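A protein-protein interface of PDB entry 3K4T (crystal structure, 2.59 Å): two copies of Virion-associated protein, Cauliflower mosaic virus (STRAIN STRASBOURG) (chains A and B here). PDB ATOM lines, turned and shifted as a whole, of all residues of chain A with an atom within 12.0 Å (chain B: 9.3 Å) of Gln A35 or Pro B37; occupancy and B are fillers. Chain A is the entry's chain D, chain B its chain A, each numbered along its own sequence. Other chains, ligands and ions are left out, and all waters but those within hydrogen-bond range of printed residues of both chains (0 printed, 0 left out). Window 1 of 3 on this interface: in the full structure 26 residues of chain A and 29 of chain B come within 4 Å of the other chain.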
ATOM      1  N   LYS A  26       2.373 -43.323  21.976  1.00  0.00           N
ATOM      2  CA  LYS A  26       1.001 -42.881  22.182  1.00  0.00           C
ATOM      3  C   LYS A  26       1.017 -41.471  22.716  1.00  0.00           C
ATOM      4  O   LYS A  26       0.170 -40.650  22.360  1.00  0.00           O
ATOM      5  CB  LYS A  26       0.332 -43.788  23.218  1.00  0.00           C
ATOM      6  CG  LYS A  26      -1.095 -44.169  22.906  1.00  0.00           C
ATOM      7  CD  LYS A  26      -1.120 -45.503  22.189  1.00  0.00           C
ATOM      8  CE  LYS A  26      -2.524 -45.856  21.738  1.00  0.00           C
ATOM      9  NZ  LYS A  26      -2.477 -46.841  20.618  1.00  0.00           N
ATOM     10  N   ALA A  27       1.989 -41.214  23.593  1.00  0.00           N
ATOM     11  CA  ALA A  27       2.199 -39.902  24.215  1.00  0.00           C
ATOM     12  C   ALA A  27       2.730 -38.861  23.221  1.00  0.00           C
ATOM     13  O   ALA A  27       2.328 -37.697  23.289  1.00  0.00           O
ATOM     14  CB  ALA A  27       3.116 -40.008  25.450  1.00  0.00           C
ATOM     15  N   ILE A  28       3.621 -39.263  22.310  1.00  0.00           N
ATOM     16  CA  ILE A  28       4.080 -38.330  21.271  1.00  0.00           C
ATOM     17  C   ILE A  28       2.849 -37.825  20.524  1.00  0.00           C
ATOM     18  O   ILE A  28       2.679 -36.622  20.334  1.00  0.00           O
ATOM     19  CB  ILE A  28       5.114 -38.950  20.294  1.00  0.00           C
ATOM     20  CG1 ILE A  28       6.474 -39.065  20.978  1.00  0.00           C
ATOM     21  CG2 ILE A  28       5.242 -38.104  19.033  1.00  0.00           C
ATOM     22  CD1 ILE A  28       7.391 -40.108  20.403  1.00  0.00           C
ATOM     23  N   LEU A  29       1.979 -38.762  20.156  1.00  0.00           N
ATOM     24  CA  LEU A  29       0.710 -38.444  19.517  1.00  0.00           C
ATOM     25  C   LEU A  29      -0.199 -37.592  20.420  1.00  0.00           C
ATOM     26  O   LEU A  29      -0.709 -36.560  19.982  1.00  0.00           O
ATOM     27  CB  LEU A  29       0.004 -39.727  19.054  1.00  0.00           C
ATOM     28  CG  LEU A  29      -1.224 -39.540  18.161  1.00  0.00           C
ATOM     29  CD1 LEU A  29      -0.837 -38.850  16.847  1.00  0.00           C
ATOM     30  CD2 LEU A  29      -1.912 -40.869  17.903  1.00  0.00           C
ATOM     31  N   GLU A  30      -0.390 -38.008  21.675  1.00  0.00           N
ATOM     32  CA  GLU A  30      -1.134 -37.203  22.656  1.00  0.00           C
ATOM     33  C   GLU A  30      -0.736 -35.728  22.545  1.00  0.00           C
ATOM     34  O   GLU A  30      -1.594 -34.864  22.404  1.00  0.00           O
ATOM     35  CB  GLU A  30      -0.881 -37.715  24.075  1.00  0.00           C
ATOM     36  CG  GLU A  30      -1.746 -38.899  24.500  1.00  0.00           C
ATOM     37  CD  GLU A  30      -2.813 -38.506  25.505  1.00  0.00           C
ATOM     38  OE1 GLU A  30      -3.102 -37.296  25.639  1.00  0.00           O
ATOM     39  OE2 GLU A  30      -3.370 -39.404  26.172  1.00  0.00           O
ATOM     40  N   LEU A  31       0.576 -35.473  22.558  1.00  0.00           N
ATOM     41  CA  LEU A  31       1.160 -34.127  22.568  1.00  0.00           C
ATOM     42  C   LEU A  31       0.923 -33.311  21.302  1.00  0.00           C
ATOM     43  O   LEU A  31       0.584 -32.121  21.383  1.00  0.00           O
ATOM     44  CB  LEU A  31       2.661 -34.205  22.854  1.00  0.00           C
ATOM     45  CG  LEU A  31       3.186 -33.640  24.169  1.00  0.00           C
ATOM     46  CD1 LEU A  31       4.533 -34.263  24.504  1.00  0.00           C
ATOM     47  CD2 LEU A  31       3.283 -32.111  24.079  1.00  0.00           C
ATOM     48  N   LEU A  32       1.122 -33.938  20.141  1.00  0.00           N
ATOM     49  CA  LEU A  32       0.863 -33.283  18.844  1.00  0.00           C
ATOM     50  C   LEU A  32      -0.655 -33.196  18.596  1.00  0.00           C
ATOM     51  O   LEU A  32      -1.094 -32.751  17.534  1.00  0.00           O
ATOM     52  CB  LEU A  32       1.572 -34.015  17.683  1.00  0.00           C
ATOM     53  CG  LEU A  32       3.062 -34.382  17.762  1.00  0.00           C
ATOM     54  CD1 LEU A  32       3.393 -35.494  16.782  1.00  0.00           C
ATOM     55  CD2 LEU A  32       3.998 -33.195  17.561  1.00  0.00           C
ATOM     56  N   GLY A  33      -1.443 -33.627  19.583  1.00  0.00           N
ATOM     57  CA  GLY A  33      -2.899 -33.493  19.554  1.00  0.00           C
ATOM     58  C   GLY A  33      -3.382 -32.369  20.454  1.00  0.00           C
ATOM     59  O   GLY A  33      -4.245 -31.584  20.061  1.00  0.00           O
ATOM     60  N   SER A  34      -2.814 -32.293  21.660  1.00  0.00           N
ATOM     61  CA  SER A  34      -3.127 -31.247  22.636  1.00  0.00           C
ATOM     62  C   SER A  34      -3.103 -29.875  21.985  1.00  0.00           C
ATOM     63  O   SER A  34      -3.733 -28.935  22.476  1.00  0.00           O
ATOM     64  CB  SER A  34      -2.184 -31.338  23.831  1.00  0.00           C
ATOM     65  OG  SER A  34      -2.352 -32.566  24.504  1.00  0.00           O
ATOM     66  N   GLN A  35      -2.351 -29.760  20.895  1.00  0.00           N
ATOM     67  CA  GLN A  35      -2.190 -28.493  20.198  1.00  0.00           C
ATOM     68  C   GLN A  35      -3.040 -28.363  18.939  1.00  0.00           C
ATOM     69  O   GLN A  35      -3.113 -29.278  18.116  1.00  0.00           O
ATOM     70  CB  GLN A  35      -0.710 -28.255  19.891  1.00  0.00           C
ATOM     71  CG  GLN A  35       0.086 -27.767  21.104  1.00  0.00           C
ATOM     72  CD  GLN A  35       1.590 -27.897  20.927  1.00  0.00           C
ATOM     73  OE1 GLN A  35       2.076 -28.814  20.257  1.00  0.00           O
ATOM     74  NE2 GLN A  35       2.335 -26.979  21.538  1.00  0.00           N
ATOM     75  N   ASN A  36      -3.690 -27.210  18.823  1.00  0.00           N
ATOM     76  CA  ASN A  36      -4.432 -26.827  17.629  1.00  0.00           C
ATOM     77  C   ASN A  36      -3.493 -26.290  16.534  1.00  0.00           C
ATOM     78  O   ASN A  36      -2.627 -25.455  16.818  1.00  0.00           O
ATOM     79  CB  ASN A  36      -5.549 -25.818  17.974  1.00  0.00           C
ATOM     80  CG  ASN A  36      -5.113 -24.749  18.994  1.00  0.00           C
ATOM     81  OD1 ASN A  36      -4.272 -24.992  19.864  1.00  0.00           O
ATOM     82  ND2 ASN A  36      -5.713 -23.567  18.893  1.00  0.00           N
ATOM     83  N   PRO A  37      -3.654 -26.786  15.285  1.00  0.00           N
ATOM     84  CA  PRO A  37      -2.820 -26.493  14.116  1.00  0.00           C
ATOM     85  C   PRO A  37      -2.245 -25.079  14.054  1.00  0.00           C
ATOM     86  O   PRO A  37      -2.936 -24.097  14.335  1.00  0.00           O
ATOM     87  CB  PRO A  37      -3.781 -26.724  12.956  1.00  0.00           C
ATOM     88  CG  PRO A  37      -4.647 -27.844  13.433  1.00  0.00           C
ATOM     89  CD  PRO A  37      -4.695 -27.775  14.946  1.00  0.00           C
ATOM     90  N   ILE A  38      -0.977 -25.003  13.669  1.00  0.00           N
ATOM     91  CA  ILE A  38      -0.225 -23.755  13.665  1.00  0.00           C
ATOM     92  C   ILE A  38      -0.852 -22.704  12.739  1.00  0.00           C
ATOM     93  O   ILE A  38      -0.908 -21.526  13.086  1.00  0.00           O
ATOM     94  CB  ILE A  38       1.268 -24.004  13.319  1.00  0.00           C
ATOM     95  CG1 ILE A  38       1.764 -25.283  14.018  1.00  0.00           C
ATOM     96  CG2 ILE A  38       2.123 -22.785  13.696  1.00  0.00           C
ATOM     97  CD1 ILE A  38       3.090 -25.847  13.491  1.00  0.00           C
ATOM     98  N   LYS A  39      -1.338 -23.140  11.579  1.00  0.00           N
ATOM     99  CA  LYS A  39      -2.007 -22.254  10.620  1.00  0.00           C
ATOM    100  C   LYS A  39      -3.378 -21.783  11.144  1.00  0.00           C
ATOM    101  O   LYS A  39      -3.849 -20.700  10.780  1.00  0.00           O
ATOM    102  CB  LYS A  39      -2.135 -22.957   9.260  1.00  0.00           C
ATOM    103  CG  LYS A  39      -2.345 -22.049   8.051  1.00  0.00           C
ATOM    104  CD  LYS A  39      -3.767 -22.154   7.508  1.00  0.00           C
ATOM    105  CE  LYS A  39      -3.829 -21.707   6.052  1.00  0.00           C
ATOM    106  NZ  LYS A  39      -5.165 -21.951   5.425  1.00  0.00           N
ATOM    107  N   GLU A  40      -3.990 -22.594  12.013  1.00  0.00           N
ATOM    108  CA  GLU A  40      -5.310 -22.307  12.601  1.00  0.00           C
ATOM    109  C   GLU A  40      -5.244 -21.266  13.726  1.00  0.00           C
ATOM    110  O   GLU A  40      -6.160 -20.452  13.879  1.00  0.00           O
ATOM    111  CB  GLU A  40      -5.953 -23.603  13.112  1.00  0.00           C
ATOM    112  CG  GLU A  40      -7.428 -23.498  13.512  1.00  0.00           C
ATOM    113  CD  GLU A  40      -8.015 -24.828  13.995  1.00  0.00           C
ATOM    114  OE1 GLU A  40      -7.242 -25.714  14.427  1.00  0.00           O
ATOM    115  OE2 GLU A  40      -9.255 -24.988  13.947  1.00  0.00           O
ATOM    116  N   SER A  41      -4.164 -21.301  14.506  1.00  0.00           N
ATOM    117  CA  SER A  41      -3.969 -20.368  15.619  1.00  0.00           C
ATOM    118  C   SER A  41      -3.432 -19.016  15.144  1.00  0.00           C
ATOM    119  O   SER A  41      -3.608 -17.996  15.817  1.00  0.00           O
ATOM    120  CB  SER A  41      -3.028 -20.973  16.666  1.00  0.00           C
ATOM    121  OG  SER A  41      -3.489 -22.238  17.120  1.00  0.00           O
ATOM    122  N   LEU A  42      -2.777 -19.017  13.986  1.00  0.00           N
ATOM    123  CA  LEU A  42      -2.211 -17.802  13.407  1.00  0.00           C
ATOM    124  C   LEU A  42      -3.274 -16.914  12.778  1.00  0.00           C
ATOM    125  O   LEU A  42      -3.128 -15.691  12.758  1.00  0.00           O
ATOM    126  CB  LEU A  42      -1.138 -18.141  12.372  1.00  0.00           C
ATOM    127  CG  LEU A  42       0.295 -18.160  12.894  1.00  0.00           C
ATOM    128  CD1 LEU A  42       1.185 -18.980  11.980  1.00  0.00           C
ATOM    129  CD2 LEU A  42       0.816 -16.737  13.017  1.00  0.00           C
ATOM    130  N   THR A  44      -6.399 -16.603  13.925  1.00  0.00           N
ATOM    131  CA  THR A  44      -7.078 -15.953  15.055  1.00  0.00           C
ATOM    132  C   THR A  44      -6.288 -14.798  15.698  1.00  0.00           C
ATOM    133  O   THR A  44      -6.863 -13.753  16.011  1.00  0.00           O
ATOM    134  CB  THR A  44      -7.517 -16.976  16.135  1.00  0.00           C
ATOM    135  OG1 THR A  44      -6.995 -18.272  15.816  1.00  0.00           O
ATOM    136  CG2 THR A  44      -9.029 -17.072  16.185  1.00  0.00           C
ATOM    137  N   VAL A  45      -4.983 -14.994  15.880  1.00  0.00           N
ATOM    138  CA  VAL A  45      -4.114 -14.002  16.523  1.00  0.00           C
ATOM    139  C   VAL A  45      -3.809 -12.835  15.575  1.00  0.00           C
ATOM    140  O   VAL A  45      -3.574 -11.704  16.023  1.00  0.00           O
ATOM    141  CB  VAL A  45      -2.819 -14.649  17.082  1.00  0.00           C
ATOM    142  CG1 VAL A  45      -1.855 -13.600  17.584  1.00  0.00           C
ATOM    143  CG2 VAL A  45      -3.152 -15.610  18.213  1.00  0.00           C
ATOM    144  N   LEU B  31      12.451 -33.450  22.653  1.00  0.00           N
ATOM    145  CA  LEU B  31      12.369 -32.357  21.686  1.00  0.00           C
ATOM    146  C   LEU B  31      11.021 -31.645  21.729  1.00  0.00           C
ATOM    147  O   LEU B  31      10.948 -30.429  21.532  1.00  0.00           O
ATOM    148  CB  LEU B  31      12.651 -32.856  20.275  1.00  0.00           C
ATOM    149  CG  LEU B  31      13.084 -31.774  19.299  1.00  0.00           C
ATOM    150  CD1 LEU B  31      14.609 -31.767  19.122  1.00  0.00           C
ATOM    151  CD2 LEU B  31      12.381 -32.001  17.983  1.00  0.00           C
ATOM    152  N   LEU B  32       9.963 -32.412  21.982  1.00  0.00           N
ATOM    153  CA  LEU B  32       8.610 -31.870  22.078  1.00  0.00           C
ATOM    154  C   LEU B  32       8.400 -31.099  23.368  1.00  0.00           C
ATOM    155  O   LEU B  32       7.698 -30.086  23.373  1.00  0.00           O
ATOM    156  CB  LEU B  32       7.575 -32.985  21.991  1.00  0.00           C
ATOM    157  CG  LEU B  32       7.396 -33.597  20.613  1.00  0.00           C
ATOM    158  CD1 LEU B  32       6.341 -34.695  20.668  1.00  0.00           C
ATOM    159  CD2 LEU B  32       7.034 -32.501  19.631  1.00  0.00           C
ATOM    160  N   GLY B  33       9.005 -31.585  24.452  1.00  0.00           N
ATOM    161  CA  GLY B  33       8.875 -30.959  25.762  1.00  0.00           C
ATOM    162  C   GLY B  33       9.957 -29.944  26.083  1.00  0.00           C
ATOM    163  O   GLY B  33      10.170 -29.612  27.251  1.00  0.00           O
ATOM    164  N   SER B  34      10.648 -29.461  25.052  1.00  0.00           N
ATOM    165  CA  SER B  34      11.653 -28.408  25.211  1.00  0.00           C
ATOM    166  C   SER B  34      11.318 -27.131  24.436  1.00  0.00           C
ATOM    167  O   SER B  34      12.116 -26.194  24.375  1.00  0.00           O
ATOM    168  CB  SER B  34      13.072 -28.968  25.069  1.00  0.00           C
ATOM    169  OG  SER B  34      13.528 -28.886  23.729  1.00  0.00           O
ATOM    170  N   GLN B  35      10.213 -27.111  23.751  1.00  0.00           N
ATOM    171  CA  GLN B  35       9.743 -25.901  23.091  1.00  0.00           C
ATOM    172  C   GLN B  35       8.509 -25.308  23.759  1.00  0.00           C
ATOM    173  O   GLN B  35       7.765 -26.017  24.442  1.00  0.00           O
ATOM    174  CB  GLN B  35       9.497 -26.218  21.606  1.00  0.00           C
ATOM    175  CG  GLN B  35       8.450 -27.299  21.319  1.00  0.00           C
ATOM    176  CD  GLN B  35       8.654 -27.995  19.979  1.00  0.00           C
ATOM    177  OE1 GLN B  35       7.841 -28.819  19.573  1.00  0.00           O
ATOM    178  NE2 GLN B  35       9.748 -27.675  19.295  1.00  0.00           N
ATOM    179  N   ASN B  36       8.314 -24.005  23.580  1.00  0.00           N
ATOM    180  CA  ASN B  36       7.167 -23.302  24.145  1.00  0.00           C
ATOM    181  C   ASN B  36       5.873 -23.655  23.393  1.00  0.00           C
ATOM    182  O   ASN B  36       5.926 -23.996  22.203  1.00  0.00           O
ATOM    183  CB  ASN B  36       7.410 -21.785  24.114  1.00  0.00           C
ATOM    184  CG  ASN B  36       8.741 -21.380  24.752  1.00  0.00           C
ATOM    185  OD1 ASN B  36       9.394 -22.177  25.425  1.00  0.00           O
ATOM    186  ND2 ASN B  36       9.144 -20.129  24.535  1.00  0.00           N
ATOM    187  N   PRO B  37       4.709 -23.593  24.082  1.00  0.00           N
ATOM    188  CA  PRO B  37       3.423 -23.751  23.385  1.00  0.00           C
ATOM    189  C   PRO B  37       3.208 -22.658  22.321  1.00  0.00           C
ATOM    190  O   PRO B  37       3.797 -21.573  22.418  1.00  0.00           O
ATOM    191  CB  PRO B  37       2.392 -23.614  24.513  1.00  0.00           C
ATOM    192  CG  PRO B  37       3.131 -23.977  25.750  1.00  0.00           C
ATOM    193  CD  PRO B  37       4.527 -23.480  25.542  1.00  0.00           C
ATOM    194  N   ILE B  38       2.377 -22.934  21.319  1.00  0.00           N
ATOM    195  CA  ILE B  38       2.151 -21.978  20.231  1.00  0.00           C
ATOM    196  C   ILE B  38       1.373 -20.725  20.683  1.00  0.00           C
ATOM    197  O   ILE B  38       1.744 -19.602  20.335  1.00  0.00           O
ATOM    198  CB  ILE B  38       1.451 -22.646  19.022  1.00  0.00           C
ATOM    199  CG1 ILE B  38       2.010 -24.055  18.793  1.00  0.00           C
ATOM    200  CG2 ILE B  38       1.629 -21.803  17.766  1.00  0.00           C
ATOM    201  CD1 ILE B  38       0.994 -25.063  18.259  1.00  0.00           C
ATOM    202  N   LYS B  39       0.314 -20.933  21.463  1.00  0.00           N
ATOM    203  CA  LYS B  39      -0.584 -19.863  21.932  1.00  0.00           C
ATOM    204  C   LYS B  39       0.109 -18.830  22.835  1.00  0.00           C
ATOM    205  O   LYS B  39      -0.211 -17.641  22.796  1.00  0.00           O
ATOM    206  CB  LYS B  39      -1.782 -20.493  22.662  1.00  0.00           C
ATOM    207  CG  LYS B  39      -2.926 -19.548  23.018  1.00  0.00           C
ATOM    208  CD  LYS B  39      -4.041 -20.315  23.713  1.00  0.00           C
ATOM    209  CE  LYS B  39      -5.171 -19.407  24.144  1.00  0.00           C
ATOM    210  NZ  LYS B  39      -6.250 -20.185  24.802  1.00  0.00           N
ATOM    211  N   GLU B  40       1.049 -19.312  23.645  1.00  0.00           N
ATOM    212  CA  GLU B  40       1.870 -18.492  24.533  1.00  0.00           C
ATOM    213  C   GLU B  40       2.886 -17.692  23.713  1.00  0.00           C
ATOM    214  O   GLU B  40       3.140 -16.519  24.000  1.00  0.00           O
ATOM    215  CB  GLU B  40       2.576 -19.398  25.557  1.00  0.00           C
ATOM    216  CG  GLU B  40       3.498 -18.714  26.565  1.00  0.00           C
ATOM    217  CD  GLU B  40       4.078 -19.692  27.589  1.00  0.00           C
ATOM    218  OE1 GLU B  40       3.505 -20.786  27.776  1.00  0.00           O
ATOM    219  OE2 GLU B  40       5.107 -19.368  28.215  1.00  0.00           O
ATOM    220  N   SER B  41       3.452 -18.343  22.696  1.00  0.00           N
ATOM    221  CA  SER B  41       4.412 -17.720  21.787  1.00  0.00           C
ATOM    222  C   SER B  41       3.730 -16.634  20.955  1.00  0.00           C
ATOM    223  O   SER B  41       4.257 -15.520  20.821  1.00  0.00           O
ATOM    224  CB  SER B  41       5.051 -18.773  20.867  1.00  0.00           C
ATOM    225  OG  SER B  41       5.763 -19.751  21.603  1.00  0.00           O
ATOM    226  N   LEU B  42       2.551 -16.962  20.420  1.00  0.00           N
ATOM    227  CA  LEU B  42       1.776 -16.048  19.575  1.00  0.00           C
ATOM    228  C   LEU B  42       1.234 -14.808  20.291  1.00  0.00           C
ATOM    229  O   LEU B  42       1.254 -13.704  19.734  1.00  0.00           O
ATOM    230  CB  LEU B  42       0.644 -16.796  18.873  1.00  0.00           C
ATOM    231  CG  LEU B  42       1.055 -17.372  17.515  1.00  0.00           C
ATOM    232  CD1 LEU B  42       0.153 -18.527  17.089  1.00  0.00           C
ATOM    233  CD2 LEU B  42       1.069 -16.269  16.464  1.00  0.00           C
ATOM    234  N   GLU B  43       0.747 -14.995  21.514  1.00  0.00           N
ATOM    235  CA  GLU B  43       0.329 -13.876  22.348  1.00  0.00           C
ATOM    236  C   GLU B  43       1.483 -12.894  22.531  1.00  0.00           C
ATOM    237  O   GLU B  43       1.311 -11.697  22.302  1.00  0.00           O
ATOM    238  CB  GLU B  43      -0.190 -14.359  23.713  1.00  0.00           C
ATOM    239  CG  GLU B  43      -1.619 -14.914  23.709  1.00  0.00           C
ATOM    240  CD  GLU B  43      -2.350 -14.671  25.027  1.00  0.00           C
ATOM    241  OE1 GLU B  43      -2.561 -13.493  25.388  1.00  0.00           O
ATOM    242  OE2 GLU B  43      -2.727 -15.655  25.699  1.00  0.00           O
ATOM    243  N   THR B  44       2.654 -13.416  22.903  1.00  0.00           N
ATOM    244  CA  THR B  44       3.828 -12.598  23.276  1.00  0.00           C
ATOM    245  C   THR B  44       4.328 -11.741  22.108  1.00  0.00           C
ATOM    246  O   THR B  44       4.703 -10.585  22.300  1.00  0.00           O
ATOM    247  CB  THR B  44       4.993 -13.473  23.876  1.00  0.00           C
ATOM    248  OG1 THR B  44       4.541 -14.160  25.053  1.00  0.00           O
ATOM    249  CG2 THR B  44       6.214 -12.632  24.234  1.00  0.00           C
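Among the printed residues, pairs that only touch across the chains: Leu A42 with Leu B42, Leu A32 with Leu B32, Val A45 with Leu B42, Gln A35 with Pro B37, Asn A36 with Ile B38, Ile A28 with Leu B32 and Gln A35 with Ile B38.
Gln A35 touches just these residues of chain B: Pro B37 and Ile B38.
Gly A33 touches none of the printed residues of chain B.
No residue of chain B comes within 4 Å of Ser A34.
Ile B38 touches just these residues of chain A: Gln A35 and Asn A36.
Of the printed residues of chain B, Ile A28 touches Leu B32 (3.9 Å).
Printed residues of chain A within 4 Å of Leu B32: Ile A28 and Leu A32.
Of the printed residues of chain B, Asn A36 touches Ile B38.
Of the printed residues of chain A, Leu B42 touches Leu A42 and Val A45.
Printed residues of chain B within 4 Å of Leu A42: Leu B42.
The nearest residue of chain B that does not touch Gln A35 is Asn B36 (4.7 Å).
Of the 14 printed residues of chain B, 4 touch a printed residue of chain A.
Hydrophobic or aromatic side chains of chain B that line the printed part of chain A: Leu B32, Ile B38 and Leu B42.
Of the 19 printed residues of chain A, 6 touch a printed residue of chain B.
Hydrophobic or aromatic side chains of chain A that line the printed part of chain B: Ile A28, Leu A32, Leu A42 and Val A45.
Among the printed residues, 7 pairs touch across the chains.
Among the printed residues, no Asp or Glu carboxylate lies within 4 Å of a Lys or Arg side-chain nitrogen of the other chain.
OG of Ser A41 sits at hydrogen-bond distance from ND2 of Asn A36.
The side-chain hydroxyl of Ser B41 is in hydrogen-bond range of the backbone carbonyl oxygen of Pro B37.
Gln A35 touches Pro B37, but with the chains exchanged Pro A37 does not touch Gln B35 (12.1 Å).
Gln A35 touches Ile B38, but with the chains exchanged Ile A38 does not touch Gln B35 (8.3 Å).
Asn A36 touches Ile B38, but with the chains exchanged Ile A38 does not touch Asn B36 (9.3 Å).
Leu A42 touches its own counterpart, Leu B42.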
